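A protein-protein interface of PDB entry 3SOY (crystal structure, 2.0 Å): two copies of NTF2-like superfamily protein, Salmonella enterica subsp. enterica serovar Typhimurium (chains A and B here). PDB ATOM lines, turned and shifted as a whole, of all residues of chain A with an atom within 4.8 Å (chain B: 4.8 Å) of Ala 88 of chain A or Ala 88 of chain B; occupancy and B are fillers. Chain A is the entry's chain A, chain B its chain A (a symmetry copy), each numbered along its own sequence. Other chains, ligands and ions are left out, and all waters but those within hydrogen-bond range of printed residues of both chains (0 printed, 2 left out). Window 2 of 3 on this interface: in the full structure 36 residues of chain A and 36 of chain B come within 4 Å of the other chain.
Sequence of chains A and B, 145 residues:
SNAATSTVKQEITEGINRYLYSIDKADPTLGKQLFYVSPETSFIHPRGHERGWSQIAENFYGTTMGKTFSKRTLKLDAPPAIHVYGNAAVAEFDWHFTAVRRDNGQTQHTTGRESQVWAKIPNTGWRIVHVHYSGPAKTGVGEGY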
ATOM      1  N   HIS A  83       6.181   5.478  22.823  1.00  0.00           N
ATOM      2  CA  HIS A  83       6.567   4.568  21.752  1.00  0.00           C
ATOM      3  C   HIS A  83       7.463   3.529  22.391  1.00  0.00           C
ATOM      4  O   HIS A  83       8.562   3.861  22.859  1.00  0.00           O
ATOM      5  CB  HIS A  83       7.370   5.338  20.716  1.00  0.00           C
ATOM      6  CG  HIS A  83       6.667   6.556  20.208  1.00  0.00           C
ATOM      7  ND1 HIS A  83       5.439   6.488  19.564  1.00  0.00           N
ATOM      8  CD2 HIS A  83       7.008   7.870  20.248  1.00  0.00           C
ATOM      9  CE1 HIS A  83       5.063   7.713  19.224  1.00  0.00           C
ATOM     10  NE2 HIS A  83       6.000   8.568  19.618  1.00  0.00           N
ATOM     11  N   VAL A  84       6.999   2.290  22.432  1.00  0.00           N
ATOM     12  CA  VAL A  84       7.737   1.212  23.078  1.00  0.00           C
ATOM     13  C   VAL A  84       8.565   0.422  22.073  1.00  0.00           C
ATOM     14  O   VAL A  84       8.050  -0.026  21.097  1.00  0.00           O
ATOM     15  CB  VAL A  84       6.778   0.243  23.759  1.00  0.00           C
ATOM     16  CG1 VAL A  84       7.562  -0.882  24.411  1.00  0.00           C
ATOM     17  CG2 VAL A  84       5.887   0.991  24.754  1.00  0.00           C
ATOM     18  N   TYR A  85       9.853   0.271  22.371  1.00  0.00           N
ATOM     19  CA  TYR A  85      10.822  -0.503  21.588  1.00  0.00           C
ATOM     20  C   TYR A  85      11.526  -1.580  22.437  1.00  0.00           C
ATOM     21  O   TYR A  85      12.721  -1.469  22.779  1.00  0.00           O
ATOM     22  CB  TYR A  85      11.870   0.459  21.026  1.00  0.00           C
ATOM     23  CG  TYR A  85      11.279   1.556  20.132  1.00  0.00           C
ATOM     24  CD1 TYR A  85      10.972   1.306  18.812  1.00  0.00           C
ATOM     25  CD2 TYR A  85      11.037   2.826  20.617  1.00  0.00           C
ATOM     26  CE1 TYR A  85      10.450   2.298  17.999  1.00  0.00           C
ATOM     27  CE2 TYR A  85      10.509   3.824  19.798  1.00  0.00           C
ATOM     28  CZ  TYR A  85      10.224   3.540  18.493  1.00  0.00           C
ATOM     29  OH  TYR A  85       9.696   4.499  17.686  1.00  0.00           O
ATOM     30  N   GLY A  86      10.770  -2.621  22.756  1.00  0.00           N
ATOM     31  CA  GLY A  86      11.273  -3.754  23.532  1.00  0.00           C
ATOM     32  C   GLY A  86      11.348  -3.315  24.969  1.00  0.00           C
ATOM     33  O   GLY A  86      10.309  -3.041  25.582  1.00  0.00           O
ATOM     34  N   ASN A  87      12.572  -3.170  25.486  1.00  0.00           N
ATOM     35  CA  ASN A  87      12.790  -2.804  26.885  1.00  0.00           C
ATOM     36  C   ASN A  87      13.227  -1.356  27.089  1.00  0.00           C
ATOM     37  O   ASN A  87      13.781  -1.002  28.122  1.00  0.00           O
ATOM     38  CB  ASN A  87      13.754  -3.787  27.542  1.00  0.00           C
ATOM     39  CG  ASN A  87      13.127  -5.181  27.731  1.00  0.00           C
ATOM     40  OD1 ASN A  87      12.040  -5.348  28.304  1.00  0.00           O
ATOM     41  ND2 ASN A  87      13.818  -6.183  27.236  1.00  0.00           N
ATOM     42  N   ALA A  88      12.933  -0.526  26.100  1.00  0.00           N
ATOM     43  CA  ALA A  88      13.124   0.899  26.187  1.00  0.00           C
ATOM     44  C   ALA A  88      11.872   1.543  25.641  1.00  0.00           C
ATOM     45  O   ALA A  88      11.117   0.923  24.888  1.00  0.00           O
ATOM     46  CB  ALA A  88      14.333   1.318  25.393  1.00  0.00           C
ATOM     47  N   ALA A  89      11.625   2.781  26.023  1.00  0.00           N
ATOM     48  CA  ALA A  89      10.477   3.503  25.496  1.00  0.00           C
ATOM     49  C   ALA A  89      10.783   4.997  25.492  1.00  0.00           C
ATOM     50  O   ALA A  89      11.561   5.495  26.347  1.00  0.00           O
ATOM     51  CB  ALA A  89       9.223   3.183  26.309  1.00  0.00           C
ATOM     52  N   VAL A  90      10.223   5.694  24.504  1.00  0.00           N
ATOM     53  CA  VAL A  90      10.345   7.129  24.392  1.00  0.00           C
ATOM     54  C   VAL A  90       8.972   7.693  24.672  1.00  0.00           C
ATOM     55  O   VAL A  90       7.986   7.279  24.053  1.00  0.00           O
ATOM     56  CB  VAL A  90      10.817   7.552  22.973  1.00  0.00           C
ATOM     57  CG1 VAL A  90      10.829   9.057  22.799  1.00  0.00           C
ATOM     58  CG2 VAL A  90      12.200   6.960  22.683  1.00  0.00           C
ATOM     59  N   TRP A 118      12.618   5.986  28.844  1.00  0.00           N
ATOM     60  CA  TRP A 118      12.449   5.004  29.919  1.00  0.00           C
ATOM     61  C   TRP A 118      13.026   3.672  29.430  1.00  0.00           C
ATOM     62  O   TRP A 118      12.882   3.307  28.237  1.00  0.00           O
ATOM     63  CB  TRP A 118      10.969   4.826  30.276  1.00  0.00           C
ATOM     64  CG  TRP A 118      10.337   6.023  30.861  1.00  0.00           C
ATOM     65  CD1 TRP A 118      10.130   7.229  30.249  1.00  0.00           C
ATOM     66  CD2 TRP A 118       9.843   6.162  32.185  1.00  0.00           C
ATOM     67  NE1 TRP A 118       9.516   8.099  31.105  1.00  0.00           N
ATOM     68  CE2 TRP A 118       9.349   7.474  32.315  1.00  0.00           C
ATOM     69  CE3 TRP A 118       9.788   5.312  33.291  1.00  0.00           C
ATOM     70  CZ2 TRP A 118       8.785   7.953  33.499  1.00  0.00           C
ATOM     71  CZ3 TRP A 118       9.237   5.813  34.497  1.00  0.00           C
ATOM     72  CH2 TRP A 118       8.743   7.113  34.582  1.00  0.00           C
ATOM     73  N   ALA A 119      13.713   2.978  30.342  1.00  0.00           N
ATOM     74  CA  ALA A 119      14.288   1.681  30.068  1.00  0.00           C
ATOM     75  C   ALA A 119      13.840   0.791  31.212  1.00  0.00           C
ATOM     76  O   ALA A 119      13.652   1.266  32.331  1.00  0.00           O
ATOM     77  CB  ALA A 119      15.804   1.746  29.984  1.00  0.00           C
ATOM     78  N   TRP A 126      10.690  -0.155  35.172  1.00  0.00           N
ATOM     79  CA  TRP A 126      10.858   0.945  34.268  1.00  0.00           C
ATOM     80  C   TRP A 126      11.292   2.197  35.006  1.00  0.00           C
ATOM     81  O   TRP A 126      10.591   2.613  35.949  1.00  0.00           O
ATOM     82  CB  TRP A 126       9.520   1.179  33.609  1.00  0.00           C
ATOM     83  CG  TRP A 126       9.224   0.082  32.581  1.00  0.00           C
ATOM     84  CD1 TRP A 126       8.535  -1.071  32.780  1.00  0.00           C
ATOM     85  CD2 TRP A 126       9.668   0.062  31.238  1.00  0.00           C
ATOM     86  NE1 TRP A 126       8.514  -1.809  31.629  1.00  0.00           N
ATOM     87  CE2 TRP A 126       9.206  -1.128  30.662  1.00  0.00           C
ATOM     88  CE3 TRP A 126      10.405   0.949  30.452  1.00  0.00           C
ATOM     89  CZ2 TRP A 126       9.464  -1.463  29.316  1.00  0.00           C
ATOM     90  CZ3 TRP A 126      10.662   0.617  29.105  1.00  0.00           C
ATOM     91  CH2 TRP A 126      10.197  -0.570  28.560  1.00  0.00           C
ATOM     92  N   HIS B  83      24.764   5.833  25.634  1.00  0.00           N
ATOM     93  CA  HIS B  83      24.402   4.992  26.767  1.00  0.00           C
ATOM     94  C   HIS B  83      23.536   3.885  26.206  1.00  0.00           C
ATOM     95  O   HIS B  83      22.429   4.153  25.717  1.00  0.00           O
ATOM     96  CB  HIS B  83      23.578   5.813  27.746  1.00  0.00           C
ATOM     97  CG  HIS B  83      24.247   7.083  28.165  1.00  0.00           C
ATOM     98  ND1 HIS B  83      25.476   7.095  28.810  1.00  0.00           N
ATOM     99  CD2 HIS B  83      23.870   8.381  28.031  1.00  0.00           C
ATOM    100  CE1 HIS B  83      25.818   8.350  29.061  1.00  0.00           C
ATOM    101  NE2 HIS B  83      24.859   9.148  28.607  1.00  0.00           N
ATOM    102  N   VAL B  84      24.033   2.660  26.253  1.00  0.00           N
ATOM    103  CA  VAL B  84      23.326   1.519  25.687  1.00  0.00           C
ATOM    104  C   VAL B  84      22.519   0.780  26.747  1.00  0.00           C
ATOM    105  O   VAL B  84      23.045   0.419  27.753  1.00  0.00           O
ATOM    106  CB  VAL B  84      24.312   0.530  25.077  1.00  0.00           C
ATOM    107  CG1 VAL B  84      23.559  -0.660  24.508  1.00  0.00           C
ATOM    108  CG2 VAL B  84      25.183   1.228  24.030  1.00  0.00           C
ATOM    109  N   TYR B  85      21.235   0.574  26.463  1.00  0.00           N
ATOM    110  CA  TYR B  85      20.287  -0.168  27.300  1.00  0.00           C
ATOM    111  C   TYR B  85      19.614  -1.322  26.531  1.00  0.00           C
ATOM    112  O   TYR B  85      18.416  -1.269  26.183  1.00  0.00           O
ATOM    113  CB  TYR B  85      19.213   0.803  27.792  1.00  0.00           C
ATOM    114  CG  TYR B  85      19.773   1.977  28.604  1.00  0.00           C
ATOM    115  CD1 TYR B  85      20.085   1.831  29.938  1.00  0.00           C
ATOM    116  CD2 TYR B  85      19.980   3.215  28.029  1.00  0.00           C
ATOM    117  CE1 TYR B  85      20.579   2.893  30.678  1.00  0.00           C
ATOM    118  CE2 TYR B  85      20.481   4.283  28.773  1.00  0.00           C
ATOM    119  CZ  TYR B  85      20.772   4.102  30.096  1.00  0.00           C
ATOM    120  OH  TYR B  85      21.273   5.131  30.831  1.00  0.00           O
ATOM    121  N   GLY B  86      20.399  -2.362  26.287  1.00  0.00           N
ATOM    122  CA  GLY B  86      19.927  -3.562  25.595  1.00  0.00           C
ATOM    123  C   GLY B  86      19.842  -3.229  24.131  1.00  0.00           C
ATOM    124  O   GLY B  86      20.873  -2.972  23.498  1.00  0.00           O
ATOM    125  N   ASN B  87      18.614  -3.156  23.606  1.00  0.00           N
ATOM    126  CA  ASN B  87      18.388  -2.897  22.183  1.00  0.00           C
ATOM    127  C   ASN B  87      17.912  -1.480  21.877  1.00  0.00           C
ATOM    128  O   ASN B  87      17.350  -1.217  20.822  1.00  0.00           O
ATOM    129  CB  ASN B  87      17.451  -3.950  21.600  1.00  0.00           C
ATOM    130  CG  ASN B  87      18.117  -5.336  21.511  1.00  0.00           C
ATOM    131  OD1 ASN B  87      19.209  -5.515  20.951  1.00  0.00           O
ATOM    132  ND2 ASN B  87      17.452  -6.319  22.078  1.00  0.00           N
ATOM    133  N   ALA B  88      18.182  -0.574  22.804  1.00  0.00           N
ATOM    134  CA  ALA B  88      17.952   0.837  22.614  1.00  0.00           C
ATOM    135  C   ALA B  88      19.186   1.552  23.111  1.00  0.00           C
ATOM    136  O   ALA B  88      19.957   1.009  23.907  1.00  0.00           O
ATOM    137  CB  ALA B  88      16.732   1.278  23.377  1.00  0.00           C
ATOM    138  N   ALA B  89      19.399   2.766  22.641  1.00  0.00           N
ATOM    139  CA  ALA B  89      20.526   3.555  23.113  1.00  0.00           C
ATOM    140  C   ALA B  89      20.180   5.036  23.011  1.00  0.00           C
ATOM    141  O   ALA B  89      19.390   5.450  22.123  1.00  0.00           O
ATOM    142  CB  ALA B  89      21.790   3.211  22.325  1.00  0.00           C
ATOM    143  N   VAL B  90      20.720   5.817  23.945  1.00  0.00           N
ATOM    144  CA  VAL B  90      20.558   7.252  23.954  1.00  0.00           C
ATOM    145  C   VAL B  90      21.916   7.832  23.632  1.00  0.00           C
ATOM    146  O   VAL B  90      22.913   7.491  24.279  1.00  0.00           O
ATOM    147  CB  VAL B  90      20.074   7.764  25.339  1.00  0.00           C
ATOM    148  CG1 VAL B  90      20.021   9.276  25.404  1.00  0.00           C
ATOM    149  CG2 VAL B  90      18.708   7.157  25.672  1.00  0.00           C
ATOM    150  N   TRP B 118      18.323   5.731  19.598  1.00  0.00           N
ATOM    151  CA  TRP B 118      18.519   4.680  18.596  1.00  0.00           C
ATOM    152  C   TRP B 118      17.978   3.370  19.180  1.00  0.00           C
ATOM    153  O   TRP B 118      18.131   3.096  20.397  1.00  0.00           O
ATOM    154  CB  TRP B 118      20.004   4.516  18.251  1.00  0.00           C
ATOM    155  CG  TRP B 118      20.604   5.685  17.581  1.00  0.00           C
ATOM    156  CD1 TRP B 118      20.777   6.937  18.105  1.00  0.00           C
ATOM    157  CD2 TRP B 118      21.095   5.742  16.250  1.00  0.00           C
ATOM    158  NE1 TRP B 118      21.368   7.760  17.187  1.00  0.00           N
ATOM    159  CE2 TRP B 118      21.553   7.054  16.026  1.00  0.00           C
ATOM    160  CE3 TRP B 118      21.174   4.816  15.208  1.00  0.00           C
ATOM    161  CZ2 TRP B 118      22.105   7.461  14.810  1.00  0.00           C
ATOM    162  CZ3 TRP B 118      21.712   5.244  13.968  1.00  0.00           C
ATOM    163  CH2 TRP B 118      22.171   6.548  13.790  1.00  0.00           C
ATOM    164  N   ALA B 119      17.311   2.595  18.322  1.00  0.00           N
ATOM    165  CA  ALA B 119      16.771   1.306  18.688  1.00  0.00           C
ATOM    166  C   ALA B 119      17.245   0.348  17.611  1.00  0.00           C
ATOM    167  O   ALA B 119      17.421   0.746  16.460  1.00  0.00           O
ATOM    168  CB  ALA B 119      15.254   1.335  18.769  1.00  0.00           C
ATOM    169  N   TRP B 126      20.423  -0.795  13.726  1.00  0.00           N
ATOM    170  CA  TRP B 126      20.224   0.363  14.549  1.00  0.00           C
ATOM    171  C   TRP B 126      19.757   1.546  13.723  1.00  0.00           C
ATOM    172  O   TRP B 126      20.447   1.913  12.752  1.00  0.00           O
ATOM    173  CB  TRP B 126      21.554   0.680  15.188  1.00  0.00           C
ATOM    174  CG  TRP B 126      21.879  -0.332  16.292  1.00  0.00           C
ATOM    175  CD1 TRP B 126      22.600  -1.477  16.175  1.00  0.00           C
ATOM    176  CD2 TRP B 126      21.435  -0.267  17.633  1.00  0.00           C
ATOM    177  NE1 TRP B 126      22.639  -2.129  17.376  1.00  0.00           N
ATOM    178  CE2 TRP B 126      21.929  -1.399  18.293  1.00  0.00           C
ATOM    179  CE3 TRP B 126      20.673   0.653  18.354  1.00  0.00           C
ATOM    180  CZ2 TRP B 126      21.679  -1.644  19.660  1.00  0.00           C
ATOM    181  CZ3 TRP B 126      20.424   0.412  19.722  1.00  0.00           C
ATOM    182  CH2 TRP B 126      20.920  -0.720  20.350  1.00  0.00           C
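Ala 88 of chain A touches Ala 88 of chain B.
Ala 88 of chain A touches one residue of chain B.
Val 90 of chain A touches none of the printed residues of chain B.
Of the printed residues of chain A, Ala 88 of chain B touches Ala 88.
Trp 126 of chain B touches none of the printed residues of chain A.
Of the 11 printed residues of chain A, 1 touches a printed residue of chain B.
Printed residues of chain A that touch a printed residue of chain B: Ala 88.
Among the printed residues, 1 pair touches across the chains.
Among the printed residues, no Asp or Glu carboxylate lies within 4 Å of a Lys or Arg side-chain nitrogen of the other chain.
Ala 88 of chain A touches its own counterpart, Ala 88 of chain B.
11 positions are printed for both chains.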
